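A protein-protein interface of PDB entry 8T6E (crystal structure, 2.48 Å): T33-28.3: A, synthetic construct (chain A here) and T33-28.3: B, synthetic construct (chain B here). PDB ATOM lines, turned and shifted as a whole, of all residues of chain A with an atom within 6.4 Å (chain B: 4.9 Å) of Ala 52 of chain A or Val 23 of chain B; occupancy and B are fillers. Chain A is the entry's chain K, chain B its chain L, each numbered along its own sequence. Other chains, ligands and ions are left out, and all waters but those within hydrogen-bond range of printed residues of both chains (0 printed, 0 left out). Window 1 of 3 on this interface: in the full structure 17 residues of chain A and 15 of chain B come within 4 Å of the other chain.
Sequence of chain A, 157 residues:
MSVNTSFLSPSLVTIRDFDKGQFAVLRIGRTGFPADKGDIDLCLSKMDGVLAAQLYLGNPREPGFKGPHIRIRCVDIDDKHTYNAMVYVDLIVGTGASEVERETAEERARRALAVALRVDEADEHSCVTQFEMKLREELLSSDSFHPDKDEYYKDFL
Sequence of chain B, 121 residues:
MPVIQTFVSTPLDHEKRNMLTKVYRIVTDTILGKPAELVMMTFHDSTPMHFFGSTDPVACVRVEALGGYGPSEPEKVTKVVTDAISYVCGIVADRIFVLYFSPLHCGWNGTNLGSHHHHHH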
ATOM      1  N   MET A  47      19.715  16.937  -2.686  1.00  0.00           N
ATOM      2  CA  MET A  47      19.737  15.519  -3.022  1.00  0.00           C
ATOM      3  C   MET A  47      18.498  15.129  -3.816  1.00  0.00           C
ATOM      4  O   MET A  47      18.590  14.395  -4.807  1.00  0.00           O
ATOM      5  CB  MET A  47      19.844  14.682  -1.747  1.00  0.00           C
ATOM      6  CG  MET A  47      21.170  14.813  -1.016  1.00  0.00           C
ATOM      7  SD  MET A  47      21.102  14.182   0.672  1.00  0.00           S
ATOM      8  CE  MET A  47      20.704  12.463   0.374  1.00  0.00           C
ATOM      9  N   ASP A  48      17.327  15.609  -3.391  1.00  0.00           N
ATOM     10  CA  ASP A  48      16.098  15.330  -4.124  1.00  0.00           C
ATOM     11  C   ASP A  48      16.118  15.981  -5.502  1.00  0.00           C
ATOM     12  O   ASP A  48      15.569  15.427  -6.460  1.00  0.00           O
ATOM     13  CB  ASP A  48      14.888  15.812  -3.319  1.00  0.00           C
ATOM     14  CG  ASP A  48      13.606  15.091  -3.693  1.00  0.00           C
ATOM     15  OD1 ASP A  48      13.449  13.922  -3.286  1.00  0.00           O
ATOM     16  OD2 ASP A  48      12.752  15.692  -4.383  1.00  0.00           O
ATOM     17  N   GLY A  49      16.756  17.148  -5.622  1.00  0.00           N
ATOM     18  CA  GLY A  49      16.846  17.798  -6.919  1.00  0.00           C
ATOM     19  C   GLY A  49      17.715  17.033  -7.898  1.00  0.00           C
ATOM     20  O   GLY A  49      17.408  16.966  -9.092  1.00  0.00           O
ATOM     21  N   VAL A  50      18.813  16.448  -7.410  1.00  0.00           N
ATOM     22  CA  VAL A  50      19.660  15.620  -8.264  1.00  0.00           C
ATOM     23  C   VAL A  50      18.902  14.390  -8.740  1.00  0.00           C
ATOM     24  O   VAL A  50      19.099  13.924  -9.869  1.00  0.00           O
ATOM     25  CB  VAL A  50      20.959  15.241  -7.522  1.00  0.00           C
ATOM     26  CG1 VAL A  50      21.800  14.286  -8.360  1.00  0.00           C
ATOM     27  CG2 VAL A  50      21.756  16.493  -7.183  1.00  0.00           C
ATOM     28  N   LEU A  51      18.012  13.853  -7.900  1.00  0.00           N
ATOM     29  CA  LEU A  51      17.168  12.741  -8.328  1.00  0.00           C
ATOM     30  C   LEU A  51      16.243  13.156  -9.466  1.00  0.00           C
ATOM     31  O   LEU A  51      15.972  12.366 -10.377  1.00  0.00           O
ATOM     32  CB  LEU A  51      16.357  12.209  -7.147  1.00  0.00           C
ATOM     33  CG  LEU A  51      16.994  11.098  -6.313  1.00  0.00           C
ATOM     34  CD1 LEU A  51      16.052  10.667  -5.201  1.00  0.00           C
ATOM     35  CD2 LEU A  51      17.364   9.916  -7.196  1.00  0.00           C
ATOM     36  N   ALA A  52      15.747  14.394  -9.428  1.00  0.00           N
ATOM     37  CA  ALA A  52      14.882  14.873 -10.501  1.00  0.00           C
ATOM     38  C   ALA A  52      15.656  15.039 -11.802  1.00  0.00           C
ATOM     39  O   ALA A  52      15.170  14.653 -12.872  1.00  0.00           O
ATOM     40  CB  ALA A  52      14.221  16.188 -10.096  1.00  0.00           C
ATOM     41  N   ALA A  53      16.863  15.609 -11.730  1.00  0.00           N
ATOM     42  CA  ALA A  53      17.677  15.775 -12.929  1.00  0.00           C
ATOM     43  C   ALA A  53      18.029  14.432 -13.555  1.00  0.00           C
ATOM     44  O   ALA A  53      18.195  14.340 -14.777  1.00  0.00           O
ATOM     45  CB  ALA A  53      18.949  16.557 -12.599  1.00  0.00           C
ATOM     46  N   GLN A  54      18.140  13.384 -12.737  1.00  0.00           N
ATOM     47  CA  GLN A  54      18.421  12.055 -13.269  1.00  0.00           C
ATOM     48  C   GLN A  54      17.314  11.590 -14.204  1.00  0.00           C
ATOM     49  O   GLN A  54      17.587  11.011 -15.263  1.00  0.00           O
ATOM     50  CB  GLN A  54      18.606  11.062 -12.121  1.00  0.00           C
ATOM     51  CG  GLN A  54      18.702   9.610 -12.564  1.00  0.00           C
ATOM     52  CD  GLN A  54      19.942   9.334 -13.388  1.00  0.00           C
ATOM     53  OE1 GLN A  54      21.065   9.424 -12.889  1.00  0.00           O
ATOM     54  NE2 GLN A  54      19.747   9.003 -14.659  1.00  0.00           N
ATOM     55  N   LEU A  55      16.057  11.846 -13.836  1.00  0.00           N
ATOM     56  CA  LEU A  55      14.936  11.417 -14.660  1.00  0.00           C
ATOM     57  C   LEU A  55      14.887  12.142 -15.998  1.00  0.00           C
ATOM     58  O   LEU A  55      14.240  11.654 -16.929  1.00  0.00           O
ATOM     59  CB  LEU A  55      13.628  11.615 -13.898  1.00  0.00           C
ATOM     60  CG  LEU A  55      13.589  10.826 -12.591  1.00  0.00           C
ATOM     61  CD1 LEU A  55      12.246  10.981 -11.901  1.00  0.00           C
ATOM     62  CD2 LEU A  55      13.902   9.361 -12.857  1.00  0.00           C
ATOM     63  N   TYR A  56      15.558  13.291 -16.116  1.00  0.00           N
ATOM     64  CA  TYR A  56      15.687  13.930 -17.420  1.00  0.00           C
ATOM     65  C   TYR A  56      16.641  13.150 -18.314  1.00  0.00           C
ATOM     66  O   TYR A  56      16.422  13.049 -19.527  1.00  0.00           O
ATOM     67  CB  TYR A  56      16.165  15.373 -17.254  1.00  0.00           C
ATOM     68  CG  TYR A  56      16.309  16.126 -18.559  1.00  0.00           C
ATOM     69  CD1 TYR A  56      15.191  16.487 -19.298  1.00  0.00           C
ATOM     70  CD2 TYR A  56      17.560  16.487 -19.045  1.00  0.00           C
ATOM     71  CE1 TYR A  56      15.313  17.178 -20.488  1.00  0.00           C
ATOM     72  CE2 TYR A  56      17.692  17.180 -20.236  1.00  0.00           C
ATOM     73  CZ  TYR A  56      16.565  17.523 -20.952  1.00  0.00           C
ATOM     74  OH  TYR A  56      16.691  18.212 -22.136  1.00  0.00           O
ATOM     75  N   LEU A  57      17.700  12.587 -17.731  1.00  0.00           N
ATOM     76  CA  LEU A  57      18.670  11.819 -18.498  1.00  0.00           C
ATOM     77  C   LEU A  57      18.196  10.401 -18.792  1.00  0.00           C
ATOM     78  O   LEU A  57      18.663   9.793 -19.761  1.00  0.00           O
ATOM     79  CB  LEU A  57      20.007  11.775 -17.755  1.00  0.00           C
ATOM     80  CG  LEU A  57      20.576  13.132 -17.332  1.00  0.00           C
ATOM     81  CD1 LEU A  57      21.925  12.963 -16.647  1.00  0.00           C
ATOM     82  CD2 LEU A  57      20.688  14.066 -18.525  1.00  0.00           C
ATOM     83  N   ALA A 112      19.593  20.305 -16.806  1.00  0.00           N
ATOM     84  CA  ALA A 112      18.677  19.778 -15.798  1.00  0.00           C
ATOM     85  C   ALA A 112      19.081  20.215 -14.395  1.00  0.00           C
ATOM     86  O   ALA A 112      18.223  20.568 -13.577  1.00  0.00           O
ATOM     87  CB  ALA A 112      18.623  18.254 -15.893  1.00  0.00           C
ATOM     88  N   ALA A 116      16.778  22.017 -11.572  1.00  0.00           N
ATOM     89  CA  ALA A 116      16.461  21.216 -10.393  1.00  0.00           C
ATOM     90  C   ALA A 116      17.124  21.755  -9.131  1.00  0.00           C
ATOM     91  O   ALA A 116      16.537  21.679  -8.046  1.00  0.00           O
ATOM     92  CB  ALA A 116      16.871  19.762 -10.622  1.00  0.00           C
ATOM     93  N   MET B  19       8.545  15.333  -6.759  1.00  0.00           N
ATOM     94  CA  MET B  19       9.503  14.806  -7.725  1.00  0.00           C
ATOM     95  C   MET B  19       9.031  15.056  -9.152  1.00  0.00           C
ATOM     96  O   MET B  19       9.803  15.514 -10.002  1.00  0.00           O
ATOM     97  CB  MET B  19       9.732  13.313  -7.487  1.00  0.00           C
ATOM     98  CG  MET B  19      10.845  12.722  -8.337  1.00  0.00           C
ATOM     99  SD  MET B  19      12.441  13.479  -7.990  1.00  0.00           S
ATOM    100  CE  MET B  19      12.679  12.976  -6.289  1.00  0.00           C
ATOM    101  N   LEU B  20       7.759  14.761  -9.431  1.00  0.00           N
ATOM    102  CA  LEU B  20       7.208  15.033 -10.754  1.00  0.00           C
ATOM    103  C   LEU B  20       7.203  16.527 -11.050  1.00  0.00           C
ATOM    104  O   LEU B  20       7.435  16.942 -12.191  1.00  0.00           O
ATOM    105  CB  LEU B  20       5.795  14.460 -10.865  1.00  0.00           C
ATOM    106  CG  LEU B  20       5.661  12.949 -10.679  1.00  0.00           C
ATOM    107  CD1 LEU B  20       4.208  12.521 -10.805  1.00  0.00           C
ATOM    108  CD2 LEU B  20       6.531  12.213 -11.684  1.00  0.00           C
ATOM    109  N   THR B  21       6.942  17.348 -10.030  1.00  0.00           N
ATOM    110  CA  THR B  21       6.960  18.796 -10.212  1.00  0.00           C
ATOM    111  C   THR B  21       8.333  19.275 -10.666  1.00  0.00           C
ATOM    112  O   THR B  21       8.448  20.068 -11.607  1.00  0.00           O
ATOM    113  CB  THR B  21       6.548  19.496  -8.916  1.00  0.00           C
ATOM    114  OG1 THR B  21       5.147  19.302  -8.688  1.00  0.00           O
ATOM    115  CG2 THR B  21       6.844  20.988  -8.993  1.00  0.00           C
ATOM    116  N   LYS B  22       9.392  18.802 -10.003  1.00  0.00           N
ATOM    117  CA  LYS B  22      10.737  19.211 -10.392  1.00  0.00           C
ATOM    118  C   LYS B  22      11.076  18.721 -11.793  1.00  0.00           C
ATOM    119  O   LYS B  22      11.698  19.447 -12.577  1.00  0.00           O
ATOM    120  CB  LYS B  22      11.766  18.700  -9.385  1.00  0.00           C
ATOM    121  CG  LYS B  22      11.522  19.144  -7.957  1.00  0.00           C
ATOM    122  CD  LYS B  22      12.800  19.092  -7.136  1.00  0.00           C
ATOM    123  CE  LYS B  22      12.487  18.956  -5.654  1.00  0.00           C
ATOM    124  NZ  LYS B  22      13.613  19.413  -4.793  1.00  0.00           N
ATOM    125  N   VAL B  23      10.678  17.491 -12.127  1.00  0.00           N
ATOM    126  CA  VAL B  23      10.908  16.984 -13.477  1.00  0.00           C
ATOM    127  C   VAL B  23      10.112  17.796 -14.491  1.00  0.00           C
ATOM    128  O   VAL B  23      10.621  18.147 -15.563  1.00  0.00           O
ATOM    129  CB  VAL B  23      10.565  15.485 -13.558  1.00  0.00           C
ATOM    130  CG1 VAL B  23      10.640  15.003 -14.998  1.00  0.00           C
ATOM    131  CG2 VAL B  23      11.503  14.676 -12.677  1.00  0.00           C
ATOM    132  N   TYR B  24       8.855  18.111 -14.168  1.00  0.00           N
ATOM    133  CA  TYR B  24       8.042  18.922 -15.069  1.00  0.00           C
ATOM    134  C   TYR B  24       8.641  20.312 -15.255  1.00  0.00           C
ATOM    135  O   TYR B  24       8.559  20.888 -16.346  1.00  0.00           O
ATOM    136  CB  TYR B  24       6.609  19.021 -14.545  1.00  0.00           C
ATOM    137  CG  TYR B  24       5.820  17.731 -14.629  1.00  0.00           C
ATOM    138  CD1 TYR B  24       6.234  16.691 -15.449  1.00  0.00           C
ATOM    139  CD2 TYR B  24       4.656  17.559 -13.891  1.00  0.00           C
ATOM    140  CE1 TYR B  24       5.515  15.513 -15.529  1.00  0.00           C
ATOM    141  CE2 TYR B  24       3.929  16.384 -13.963  1.00  0.00           C
ATOM    142  CZ  TYR B  24       4.363  15.364 -14.784  1.00  0.00           C
ATOM    143  OH  TYR B  24       3.646  14.192 -14.862  1.00  0.00           O
ATOM    144  N   ARG B  25       9.244  20.870 -14.200  1.00  0.00           N
ATOM    145  CA  ARG B  25       9.928  22.152 -14.340  1.00  0.00           C
ATOM    146  C   ARG B  25      11.117  22.039 -15.287  1.00  0.00           C
ATOM    147  O   ARG B  25      11.417  22.976 -16.034  1.00  0.00           O
ATOM    148  CB  ARG B  25      10.378  22.670 -12.971  1.00  0.00           C
ATOM    149  CG  ARG B  25       9.255  23.261 -12.130  1.00  0.00           C
ATOM    150  CD  ARG B  25       9.740  23.772 -10.776  1.00  0.00           C
ATOM    151  NE  ARG B  25      10.678  24.884 -10.888  1.00  0.00           N
ATOM    152  CZ  ARG B  25      11.950  24.833 -10.518  1.00  0.00           C
ATOM    153  NH1 ARG B  25      12.474  23.737  -9.993  1.00  0.00           N
ATOM    154  NH2 ARG B  25      12.715  25.911 -10.670  1.00  0.00           N
ATOM    155  N   ILE B  26      11.805  20.896 -15.269  1.00  0.00           N
ATOM    156  CA  ILE B  26      12.914  20.682 -16.193  1.00  0.00           C
ATOM    157  C   ILE B  26      12.398  20.550 -17.620  1.00  0.00           C
ATOM    158  O   ILE B  26      12.945  21.147 -18.554  1.00  0.00           O
ATOM    159  CB  ILE B  26      13.728  19.444 -15.774  1.00  0.00           C
ATOM    160  CG1 ILE B  26      14.285  19.623 -14.360  1.00  0.00           C
ATOM    161  CG2 ILE B  26      14.851  19.187 -16.765  1.00  0.00           C
ATOM    162  CD1 ILE B  26      14.815  18.344 -13.745  1.00  0.00           C
ATOM    163  N   VAL B  27      11.334  19.764 -17.808  1.00  0.00           N
ATOM    164  CA  VAL B  27      10.773  19.558 -19.141  1.00  0.00           C
ATOM    165  C   VAL B  27      10.299  20.879 -19.732  1.00  0.00           C
ATOM    166  O   VAL B  27      10.465  21.137 -20.931  1.00  0.00           O
ATOM    167  CB  VAL B  27       9.633  18.524 -19.085  1.00  0.00           C
ATOM    168  CG1 VAL B  27       8.964  18.389 -20.446  1.00  0.00           C
ATOM    169  CG2 VAL B  27      10.159  17.180 -18.614  1.00  0.00           C
ATOM    170  N   VAL B  80      10.786  11.763 -21.285  1.00  0.00           N
ATOM    171  CA  VAL B  80      11.124  12.196 -19.932  1.00  0.00           C
ATOM    172  C   VAL B  80       9.953  11.963 -18.984  1.00  0.00           C
ATOM    173  O   VAL B  80      10.140  11.527 -17.841  1.00  0.00           O
ATOM    174  CB  VAL B  80      11.564  13.673 -19.933  1.00  0.00           C
ATOM    175  CG1 VAL B  80      12.033  14.089 -18.546  1.00  0.00           C
ATOM    176  CG2 VAL B  80      12.662  13.902 -20.961  1.00  0.00           C
ATOM    177  N   ALA B  84       9.931   9.540 -15.782  1.00  0.00           N
ATOM    178  CA  ALA B  84       9.658  10.068 -14.448  1.00  0.00           C
ATOM    179  C   ALA B  84       8.474   9.358 -13.804  1.00  0.00           C
ATOM    180  O   ALA B  84       8.537   8.964 -12.633  1.00  0.00           O
ATOM    181  CB  ALA B  84       9.407  11.572 -14.522  1.00  0.00           C
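NZ of Lys 22 of chain B lies within salt-bridge range of OD2 of Asp 48 of chain A (3.8 Å). The side-chain sulfur (SD) of Met 19 of chain B sits at hydrogen-bond distance from the backbone NH (N) of Ala 52 of chain A, 3.7 Å away.
CE of Met 19 of chain B touches OD1 of Asp 48 of chain A, 3.2 Å away. Ala 52 of chain A touches Lys 22 of chain B (CB to CB, 3.6 Å). Val 23 of chain B touches Ala 52 of chain A (CG2 to O, 3.7 Å). Leu 55 of chain A touches Val 23 of chain B (CD1 to CG2, 3.8 Å). O of Leu 55 of chain A touches CG1 of Val 80 of chain B, 3.7 Å away. Leu 55 of chain A touches Ala 84 of chain B. Tyr 56 of chain A touches Ile 26 of chain B (CD1 to CG2, 3.7 Å). CA of Tyr 56 of chain A touches CG1 of Val 80 of chain B, at 3.8 Å. Ile 26 of chain B touches Ala 112 of chain A (CG2 to CB, 3.98 Å). CB of Ala 116 of chain A touches CD1 of Ile 26 of chain B, at 3.999 Å.
Of the printed residues of chain B, Leu 51 of chain A touches Met 19. Ala 52 of chain A touches four residues of chain B. Of the printed residues of chain B, Tyr 56 of chain A touches Ile 26 (3.7 Å) and Val 80 (3.8 Å). Val 23 of chain B touches just these residues of chain A: Ala 52 and Leu 55. The nearest printed residue of chain B that does not touch Ala 52 of chain A is Val 80 of chain B (6.5 Å). The nearest residue of chain A that does not touch Val 23 of chain B is Tyr 56 of chain A (5.3 Å). The nearest printed residue of chain A that does not touch Ile 26 of chain B is Gly 49 of chain A (5.5 Å).
Of the 11 printed residues of chain B, 6 touch a printed residue of chain A. Hydrophobic or aromatic side chains of chain B within 4 Å of the printed part of chain A: Met 19, Val 23, Ile 26, Val 80 and Ala 84. Among the printed residues, Asp or Glu carboxylates within 4 Å of a Lys or Arg side-chain nitrogen of the other chain: Asp 48 of chain A with Lys 22 of chain B.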
